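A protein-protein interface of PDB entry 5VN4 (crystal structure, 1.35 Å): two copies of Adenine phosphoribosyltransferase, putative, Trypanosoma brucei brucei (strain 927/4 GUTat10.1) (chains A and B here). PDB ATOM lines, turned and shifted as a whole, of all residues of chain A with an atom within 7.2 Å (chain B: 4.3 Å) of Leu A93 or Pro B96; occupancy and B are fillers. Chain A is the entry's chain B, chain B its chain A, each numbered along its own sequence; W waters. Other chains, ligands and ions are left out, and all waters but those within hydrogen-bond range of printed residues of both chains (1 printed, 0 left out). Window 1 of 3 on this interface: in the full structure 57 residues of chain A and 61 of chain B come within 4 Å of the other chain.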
ATOM      1  N   VAL A  53      10.598  -8.120  10.065  1.00  0.00           N
ATOM      2  CA  VAL A  53      10.662  -8.700  11.403  1.00  0.00           C
ATOM      3  C   VAL A  53      11.245  -7.729  12.424  1.00  0.00           C
ATOM      4  O   VAL A  53      10.988  -7.874  13.624  1.00  0.00           O
ATOM      5  CB  VAL A  53      11.422 -10.042  11.389  1.00  0.00           C
ATOM      6  CG1 VAL A  53      12.925  -9.806  11.321  1.00  0.00           C
ATOM      7  CG2 VAL A  53      11.045 -10.898  12.606  1.00  0.00           C
ATOM      8  N   GLY A  54      12.021  -6.733  11.985  1.00  0.00           N
ATOM      9  CA  GLY A  54      12.635  -5.823  12.936  1.00  0.00           C
ATOM     10  C   GLY A  54      11.634  -5.037  13.763  1.00  0.00           C
ATOM     11  O   GLY A  54      11.928  -4.650  14.896  1.00  0.00           O
ATOM     12  N   THR A  57      10.963  -7.461  16.685  1.00  0.00           N
ATOM     13  CA  THR A  57      12.030  -7.585  17.676  1.00  0.00           C
ATOM     14  C   THR A  57      12.232  -6.291  18.451  1.00  0.00           C
ATOM     15  O   THR A  57      12.700  -6.322  19.595  1.00  0.00           O
ATOM     16  CB  THR A  57      13.343  -8.062  17.040  1.00  0.00           C
ATOM     17  OG1 THR A  57      13.824  -7.083  16.109  1.00  0.00           O
ATOM     18  CG2 THR A  57      13.131  -9.389  16.324  1.00  0.00           C
ATOM     19  N   MET A  63       7.610  -9.585  21.754  1.00  0.00           N
ATOM     20  CA  MET A  63       8.583 -10.673  21.847  1.00  0.00           C
ATOM     21  C   MET A  63       8.301 -11.553  23.060  1.00  0.00           C
ATOM     22  O   MET A  63       8.358 -12.785  22.972  1.00  0.00           O
ATOM     23  CB  MET A  63      10.002 -10.105  21.886  1.00  0.00           C
ATOM     24  CG  MET A  63      10.435  -9.493  20.570  1.00  0.00           C
ATOM     25  SD  MET A  63      10.723 -10.741  19.287  1.00  0.00           S
ATOM     26  CE  MET A  63      12.335 -11.378  19.767  1.00  0.00           C
ATOM     27  N   ARG A  67       7.307 -15.536  23.004  1.00  0.00           N
ATOM     28  CA  ARG A  67       8.029 -16.507  23.816  1.00  0.00           C
ATOM     29  C   ARG A  67       7.085 -17.224  24.773  1.00  0.00           C
ATOM     30  O   ARG A  67       7.083 -18.456  24.857  1.00  0.00           O
ATOM     31  CB  ARG A  67       9.132 -15.797  24.591  1.00  0.00           C
ATOM     32  CG  ARG A  67       9.939 -16.757  25.416  1.00  0.00           C
ATOM     33  CD  ARG A  67      10.683 -16.048  26.490  1.00  0.00           C
ATOM     34  NE  ARG A  67       9.791 -15.442  27.472  1.00  0.00           N
ATOM     35  CZ  ARG A  67      10.234 -14.751  28.511  1.00  0.00           C
ATOM     36  NH1 ARG A  67      11.539 -14.601  28.676  1.00  0.00           N
ATOM     37  NH2 ARG A  67       9.388 -14.214  29.375  1.00  0.00           N
ATOM     38  N   PHE A  87      15.365 -21.534  11.630  1.00  0.00           N
ATOM     39  CA  PHE A  87      15.966 -21.205  10.339  1.00  0.00           C
ATOM     40  C   PHE A  87      16.773 -19.908  10.355  1.00  0.00           C
ATOM     41  O   PHE A  87      16.348 -18.885  10.894  1.00  0.00           O
ATOM     42  CB  PHE A  87      14.897 -21.094   9.248  1.00  0.00           C
ATOM     43  CG  PHE A  87      14.212 -22.390   8.926  1.00  0.00           C
ATOM     44  CD1 PHE A  87      14.731 -23.250   7.964  1.00  0.00           C
ATOM     45  CD2 PHE A  87      13.037 -22.751   9.575  1.00  0.00           C
ATOM     46  CE1 PHE A  87      14.088 -24.440   7.657  1.00  0.00           C
ATOM     47  CE2 PHE A  87      12.397 -23.933   9.269  1.00  0.00           C
ATOM     48  CZ  PHE A  87      12.918 -24.780   8.305  1.00  0.00           C
ATOM     49  N   SER A  89      17.815 -16.629   8.741  1.00  0.00           N
ATOM     50  CA  SER A  89      18.365 -15.917   9.893  1.00  0.00           C
ATOM     51  C   SER A  89      17.260 -15.464  10.854  1.00  0.00           C
ATOM     52  O   SER A  89      17.515 -15.132  12.009  1.00  0.00           O
ATOM     53  CB  SER A  89      19.064 -14.637   9.406  1.00  0.00           C
ATOM     54  OG  SER A  89      19.913 -14.869   8.289  1.00  0.00           O
ATOM     55  N   ARG A  90      16.038 -15.343  10.337  1.00  0.00           N
ATOM     56  CA  ARG A  90      14.989 -14.743  11.156  1.00  0.00           C
ATOM     57  C   ARG A  90      14.417 -15.720  12.179  1.00  0.00           C
ATOM     58  O   ARG A  90      13.973 -15.292  13.250  1.00  0.00           O
ATOM     59  CB  ARG A  90      13.916 -14.097  10.279  1.00  0.00           C
ATOM     60  CG  ARG A  90      14.452 -12.940   9.447  1.00  0.00           C
ATOM     61  CD  ARG A  90      13.329 -12.237   8.725  1.00  0.00           C
ATOM     62  NE  ARG A  90      13.425 -12.338   7.277  1.00  0.00           N
ATOM     63  CZ  ARG A  90      12.369 -12.299   6.469  1.00  0.00           C
ATOM     64  NH1 ARG A  90      11.138 -12.196   6.981  1.00  0.00           N
ATOM     65  NH2 ARG A  90      12.539 -12.378   5.155  1.00  0.00           N
ATOM     66  N   GLY A  91      14.442 -17.023  11.888  1.00  0.00           N
ATOM     67  CA  GLY A  91      14.087 -17.999  12.906  1.00  0.00           C
ATOM     68  C   GLY A  91      15.024 -17.956  14.096  1.00  0.00           C
ATOM     69  O   GLY A  91      14.628 -18.277  15.221  1.00  0.00           O
ATOM     70  N   PHE A  92      16.280 -17.554  13.867  1.00  0.00           N
ATOM     71  CA  PHE A  92      17.244 -17.395  14.951  1.00  0.00           C
ATOM     72  C   PHE A  92      16.792 -16.368  15.977  1.00  0.00           C
ATOM     73  O   PHE A  92      17.250 -16.413  17.122  1.00  0.00           O
ATOM     74  CB  PHE A  92      18.584 -16.892  14.411  1.00  0.00           C
ATOM     75  CG  PHE A  92      19.381 -17.908  13.626  1.00  0.00           C
ATOM     76  CD1 PHE A  92      18.911 -19.194  13.368  1.00  0.00           C
ATOM     77  CD2 PHE A  92      20.640 -17.553  13.155  1.00  0.00           C
ATOM     78  CE1 PHE A  92      19.682 -20.091  12.660  1.00  0.00           C
ATOM     79  CE2 PHE A  92      21.420 -18.443  12.446  1.00  0.00           C
ATOM     80  CZ  PHE A  92      20.938 -19.713  12.190  1.00  0.00           C
ATOM     81  N   LEU A  93      15.937 -15.416  15.585  1.00  0.00           N
ATOM     82  CA  LEU A  93      15.477 -14.367  16.490  1.00  0.00           C
ATOM     83  C   LEU A  93      14.440 -14.858  17.485  1.00  0.00           C
ATOM     84  O   LEU A  93      14.226 -14.201  18.509  1.00  0.00           O
ATOM     85  CB  LEU A  93      14.859 -13.219  15.687  1.00  0.00           C
ATOM     86  CG  LEU A  93      15.823 -12.483  14.763  1.00  0.00           C
ATOM     87  CD1 LEU A  93      15.042 -11.687  13.720  1.00  0.00           C
ATOM     88  CD2 LEU A  93      16.753 -11.582  15.569  1.00  0.00           C
ATOM     89  N   LEU A  94      13.792 -15.986  17.208  1.00  0.00           N
ATOM     90  CA  LEU A  94      12.650 -16.453  17.985  1.00  0.00           C
ATOM     91  C   LEU A  94      12.932 -17.724  18.771  1.00  0.00           C
ATOM     92  O   LEU A  94      12.464 -17.862  19.904  1.00  0.00           O
ATOM     93  CB  LEU A  94      11.458 -16.695  17.056  1.00  0.00           C
ATOM     94  CG  LEU A  94      11.070 -15.513  16.165  1.00  0.00           C
ATOM     95  CD1 LEU A  94       9.928 -15.899  15.233  1.00  0.00           C
ATOM     96  CD2 LEU A  94      10.688 -14.289  16.999  1.00  0.00           C
ATOM     97  N   GLY A  95      13.684 -18.659  18.202  1.00  0.00           N
ATOM     98  CA  GLY A  95      13.866 -19.958  18.806  1.00  0.00           C
ATOM     99  C   GLY A  95      14.613 -19.961  20.128  1.00  0.00           C
ATOM    100  O   GLY A  95      14.183 -20.612  21.087  1.00  0.00           O
ATOM    101  N   PRO A  96      15.762 -19.266  20.204  1.00  0.00           N
ATOM    102  CA  PRO A  96      16.554 -19.319  21.447  1.00  0.00           C
ATOM    103  C   PRO A  96      15.808 -18.887  22.699  1.00  0.00           C
ATOM    104  O   PRO A  96      15.939 -19.547  23.738  1.00  0.00           O
ATOM    105  CB  PRO A  96      17.760 -18.427  21.128  1.00  0.00           C
ATOM    106  CG  PRO A  96      17.938 -18.607  19.670  1.00  0.00           C
ATOM    107  CD  PRO A  96      16.540 -18.643  19.114  1.00  0.00           C
ATOM    108  N   MET A  97      15.020 -17.809  22.641  1.00  0.00           N
ATOM    109  CA  MET A  97      14.346 -17.365  23.857  1.00  0.00           C
ATOM    110  C   MET A  97      13.327 -18.388  24.333  1.00  0.00           C
ATOM    111  O   MET A  97      13.075 -18.490  25.539  1.00  0.00           O
ATOM    112  CB  MET A  97      13.715 -15.986  23.681  1.00  0.00           C
ATOM    113  CG  MET A  97      12.533 -15.951  22.744  1.00  0.00           C
ATOM    114  SD  MET A  97      12.043 -14.251  22.392  1.00  0.00           S
ATOM    115  CE  MET A  97      10.699 -14.550  21.242  1.00  0.00           C
ATOM    116  N   ILE A  98      12.755 -19.163  23.410  1.00  0.00           N
ATOM    117  CA  ILE A  98      11.845 -20.241  23.786  1.00  0.00           C
ATOM    118  C   ILE A  98      12.630 -21.432  24.326  1.00  0.00           C
ATOM    119  O   ILE A  98      12.290 -21.993  25.376  1.00  0.00           O
ATOM    120  CB  ILE A  98      10.971 -20.626  22.580  1.00  0.00           C
ATOM    121  CG1 ILE A  98      10.062 -19.458  22.187  1.00  0.00           C
ATOM    122  CG2 ILE A  98      10.155 -21.894  22.874  1.00  0.00           C
ATOM    123  CD1 ILE A  98       9.514 -19.581  20.791  1.00  0.00           C
ATOM    124  N   PHE A 106      18.720 -25.440  21.182  1.00  0.00           N
ATOM    125  CA  PHE A 106      18.314 -24.768  19.954  1.00  0.00           C
ATOM    126  C   PHE A 106      19.297 -25.159  18.859  1.00  0.00           C
ATOM    127  O   PHE A 106      20.506 -24.949  19.004  1.00  0.00           O
ATOM    128  CB  PHE A 106      18.262 -23.245  20.100  1.00  0.00           C
ATOM    129  CG  PHE A 106      17.866 -22.552  18.835  1.00  0.00           C
ATOM    130  CD1 PHE A 106      16.556 -22.622  18.377  1.00  0.00           C
ATOM    131  CD2 PHE A 106      18.806 -21.901  18.067  1.00  0.00           C
ATOM    132  CE1 PHE A 106      16.182 -22.022  17.186  1.00  0.00           C
ATOM    133  CE2 PHE A 106      18.441 -21.291  16.883  1.00  0.00           C
ATOM    134  CZ  PHE A 106      17.128 -21.354  16.438  1.00  0.00           C
ATOM    135  N   ASP A 155      10.035 -17.089  11.265  1.00  0.00           N
ATOM    136  CA  ASP A 155       9.125 -15.960  11.462  1.00  0.00           C
ATOM    137  C   ASP A 155       7.899 -16.065  10.557  1.00  0.00           C
ATOM    138  O   ASP A 155       6.764 -16.099  11.042  1.00  0.00           O
ATOM    139  CB  ASP A 155       9.830 -14.592  11.367  1.00  0.00           C
ATOM    140  CG  ASP A 155      10.335 -14.249   9.966  1.00  0.00           C
ATOM    141  OD1 ASP A 155      10.760 -15.155   9.220  1.00  0.00           O
ATOM    142  OD2 ASP A 155      10.339 -13.044   9.624  1.00  0.00           O
ATOM    143  N   PHE B  92      22.028 -12.498  16.271  1.00  0.00           N
ATOM    144  CA  PHE B  92      20.588 -12.698  16.417  1.00  0.00           C
ATOM    145  C   PHE B  92      20.266 -13.791  17.423  1.00  0.00           C
ATOM    146  O   PHE B  92      19.172 -13.796  17.994  1.00  0.00           O
ATOM    147  CB  PHE B  92      19.983 -13.123  15.075  1.00  0.00           C
ATOM    148  CG  PHE B  92      19.845 -12.011  14.054  1.00  0.00           C
ATOM    149  CD1 PHE B  92      20.344 -10.731  14.271  1.00  0.00           C
ATOM    150  CD2 PHE B  92      19.183 -12.270  12.864  1.00  0.00           C
ATOM    151  CE1 PHE B  92      20.172  -9.732  13.316  1.00  0.00           C
ATOM    152  CE2 PHE B  92      19.009 -11.281  11.907  1.00  0.00           C
ATOM    153  CZ  PHE B  92      19.510 -10.008  12.129  1.00  0.00           C
ATOM    154  N   LEU B  94      21.680 -14.342  20.293  1.00  0.00           N
ATOM    155  CA  LEU B  94      22.014 -13.966  21.660  1.00  0.00           C
ATOM    156  C   LEU B  94      21.254 -12.745  22.157  1.00  0.00           C
ATOM    157  O   LEU B  94      20.876 -12.697  23.327  1.00  0.00           O
ATOM    158  CB  LEU B  94      23.525 -13.704  21.777  1.00  0.00           C
ATOM    159  CG  LEU B  94      24.441 -14.842  21.320  1.00  0.00           C
ATOM    160  CD1 LEU B  94      25.910 -14.406  21.347  1.00  0.00           C
ATOM    161  CD2 LEU B  94      24.219 -16.087  22.174  1.00  0.00           C
ATOM    162  N   GLY B  95      21.046 -11.738  21.310  1.00  0.00           N
ATOM    163  CA  GLY B  95      20.442 -10.491  21.729  1.00  0.00           C
ATOM    164  C   GLY B  95      19.012 -10.578  22.238  1.00  0.00           C
ATOM    165  O   GLY B  95      18.689 -10.045  23.306  1.00  0.00           O
ATOM    166  N   PRO B  96      18.118 -11.231  21.482  1.00  0.00           N
ATOM    167  CA  PRO B  96      16.696 -11.211  21.874  1.00  0.00           C
ATOM    168  C   PRO B  96      16.411 -11.754  23.262  1.00  0.00           C
ATOM    169  O   PRO B  96      15.576 -11.180  23.974  1.00  0.00           O
ATOM    170  CB  PRO B  96      16.021 -12.034  20.769  1.00  0.00           C
ATOM    171  CG  PRO B  96      16.873 -11.788  19.575  1.00  0.00           C
ATOM    172  CD  PRO B  96      18.284 -11.781  20.125  1.00  0.00           C
ATOM    173  N   MET B  97      17.070 -12.839  23.678  1.00  0.00           N
ATOM    174  CA  MET B  97      16.775 -13.385  25.003  1.00  0.00           C
ATOM    175  C   MET B  97      17.215 -12.438  26.112  1.00  0.00           C
ATOM    176  O   MET B  97      16.651 -12.472  27.210  1.00  0.00           O
ATOM    177  CB  MET B  97      17.408 -14.767  25.178  1.00  0.00           C
ATOM    178  CG  MET B  97      18.935 -14.760  25.271  1.00  0.00           C
ATOM    179  SD  MET B  97      19.586 -16.440  25.225  1.00  0.00           S
ATOM    180  CE  MET B  97      21.339 -16.091  25.279  1.00  0.00           C
ATOM    181  N   ILE B  98      18.211 -11.593  25.847  1.00  0.00           N
ATOM    182  CA  ILE B  98      18.615 -10.571  26.809  1.00  0.00           C
ATOM    183  C   ILE B  98      17.649  -9.397  26.776  1.00  0.00           C
ATOM    184  O   ILE B  98      17.163  -8.941  27.819  1.00  0.00           O
ATOM    185  CB  ILE B  98      20.066 -10.132  26.531  1.00  0.00           C
ATOM    186  CG1 ILE B  98      21.015 -11.323  26.688  1.00  0.00           C
ATOM    187  CG2 ILE B  98      20.471  -8.986  27.455  1.00  0.00           C
ATOM    188  CD1 ILE B  98      22.364 -11.118  26.011  1.00  0.00           C
ATOM    189  N   ALA B  99      17.331  -8.923  25.566  1.00  0.00           N
ATOM    190  CA  ALA B  99      16.474  -7.753  25.409  1.00  0.00           C
ATOM    191  C   ALA B  99      15.090  -7.969  26.011  1.00  0.00           C
ATOM    192  O   ALA B  99      14.507  -7.042  26.584  1.00  0.00           O
ATOM    193  CB  ALA B  99      16.352  -7.393  23.930  1.00  0.00           C
ATOM    194  N   VAL B 100      14.533  -9.179  25.883  1.00  0.00           N
ATOM    195  CA  VAL B 100      13.193  -9.402  26.409  1.00  0.00           C
ATOM    196  C   VAL B 100      13.174  -9.263  27.927  1.00  0.00           C
ATOM    197  O   VAL B 100      12.228  -8.701  28.490  1.00  0.00           O
ATOM    198  CB  VAL B 100      12.597 -10.730  25.899  1.00  0.00           C
ATOM    199  CG1 VAL B 100      13.303 -11.927  26.511  1.00  0.00           C
ATOM    200  CG2 VAL B 100      11.099 -10.777  26.165  1.00  0.00           C
ATOM    201  N   PHE B 106      15.190  -5.016  20.610  1.00  0.00           N
ATOM    202  CA  PHE B 106      16.315  -5.631  19.923  1.00  0.00           C
ATOM    203  C   PHE B 106      16.298  -5.151  18.479  1.00  0.00           C
ATOM    204  O   PHE B 106      15.319  -5.369  17.756  1.00  0.00           O
ATOM    205  CB  PHE B 106      16.280  -7.156  19.979  1.00  0.00           C
ATOM    206  CG  PHE B 106      17.442  -7.770  19.273  1.00  0.00           C
ATOM    207  CD1 PHE B 106      18.719  -7.648  19.794  1.00  0.00           C
ATOM    208  CD2 PHE B 106      17.275  -8.404  18.058  1.00  0.00           C
ATOM    209  CE1 PHE B 106      19.810  -8.188  19.132  1.00  0.00           C
ATOM    210  CE2 PHE B 106      18.356  -8.948  17.395  1.00  0.00           C
ATOM    211  CZ  PHE B 106      19.624  -8.836  17.930  1.00  0.00           C
ATOM    212  N   LEU B 108      17.996  -4.904  14.649  1.00  0.00           N
ATOM    213  CA  LEU B 108      18.752  -5.753  13.736  1.00  0.00           C
ATOM    214  C   LEU B 108      19.799  -4.949  12.977  1.00  0.00           C
ATOM    215  O   LEU B 108      19.483  -3.930  12.359  1.00  0.00           O
ATOM    216  CB  LEU B 108      17.816  -6.418  12.724  1.00  0.00           C
ATOM    217  CG  LEU B 108      16.553  -7.079  13.258  1.00  0.00           C
ATOM    218  CD1 LEU B 108      15.844  -7.802  12.130  1.00  0.00           C
ATOM    219  CD2 LEU B 108      16.889  -8.020  14.394  1.00  0.00           C
HETATM  220  O   HOH W   1      17.475 -15.169  19.491  1.00  0.00           O
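Phe A92 touches its own counterpart, Phe B92.
The backbone carbonyl oxygen (O) of Gly A54 lies within hydrogen-bond range of the side-chain hydroxyl (OG1) of Thr A57, 3.3 Å away. N of Phe A92 sits at hydrogen-bond distance from O of Phe A87, 3.3 Å away.
Leu B108 touches Val A53. CD1 of Leu B108 touches CA of Gly A54, at 3.9 Å. Leu B108 touches Thr A57 (CD2 to OG1, 3.6 Å). Met A63 touches Pro B96. CG1 of Val B100 touches NH1 of Arg A67, 3.9 Å away. O of Ser A89 touches CD2 of Phe B92, 3.4 Å away. CG of Phe B92 touches CD2 of Leu A93, 3.5 Å away. Leu A93 touches Pro B96. Phe B106 touches Leu A93. Leu A93 touches Leu B108 (CD2 to CD2, 3.8 Å).
OG1 of Thr A57 sits at hydrogen-bond distance from O of Phe B106 (2.8 Å). O of Phe A92 sits close to O of Phe B92 (3.4 Å).
Of chain B, only Phe B92 (3.5 Å), Pro B96 (3.6 Å), Phe B106 (3.6 Å) and Leu B108 (3.8 Å) come within 4 Å of Leu A93. Gly B95 touches none of the printed residues of chain A. Of the printed residues of chain B, Ser A89 touches Phe B92 (3.4 Å). Of the printed residues of chain B, Arg A67 touches Val B100 (3.9 Å). Of the printed residues of chain A, Leu B108 touches Val A53 (3.6 Å), Gly A54 (3.9 Å), Thr A57 (3.6 Å) and Leu A93 (3.8 Å). Leu A94 touches none of the printed residues of chain B.
Printed residues of chain B that touch a printed residue of chain A: Phe B92, Pro B96, Val B100, Phe B106 and Leu B108. Hydrophobic or aromatic side chains of chain B within 4 Å of the printed part of chain A: Phe B92, Pro B96, Val B100, Phe B106 and Leu B108. Hydrophobic or aromatic side chains of chain A within 4 Å of the printed part of chain B: Val A53, Met A63 and Leu A93. Along chain A the printed residues that touch a printed residue of chain B span positions 53 to 93. Among the printed residues, 12 pairs touch across the chains. Among the printed residues, no Asp or Glu carboxylate lies within 4 Å of a Lys or Arg side-chain nitrogen of the other chain.
Water W1 lies within hydrogen-bond range of O of Phe B92 (2.6 Å) and O of Phe A92 (2.7 Å).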
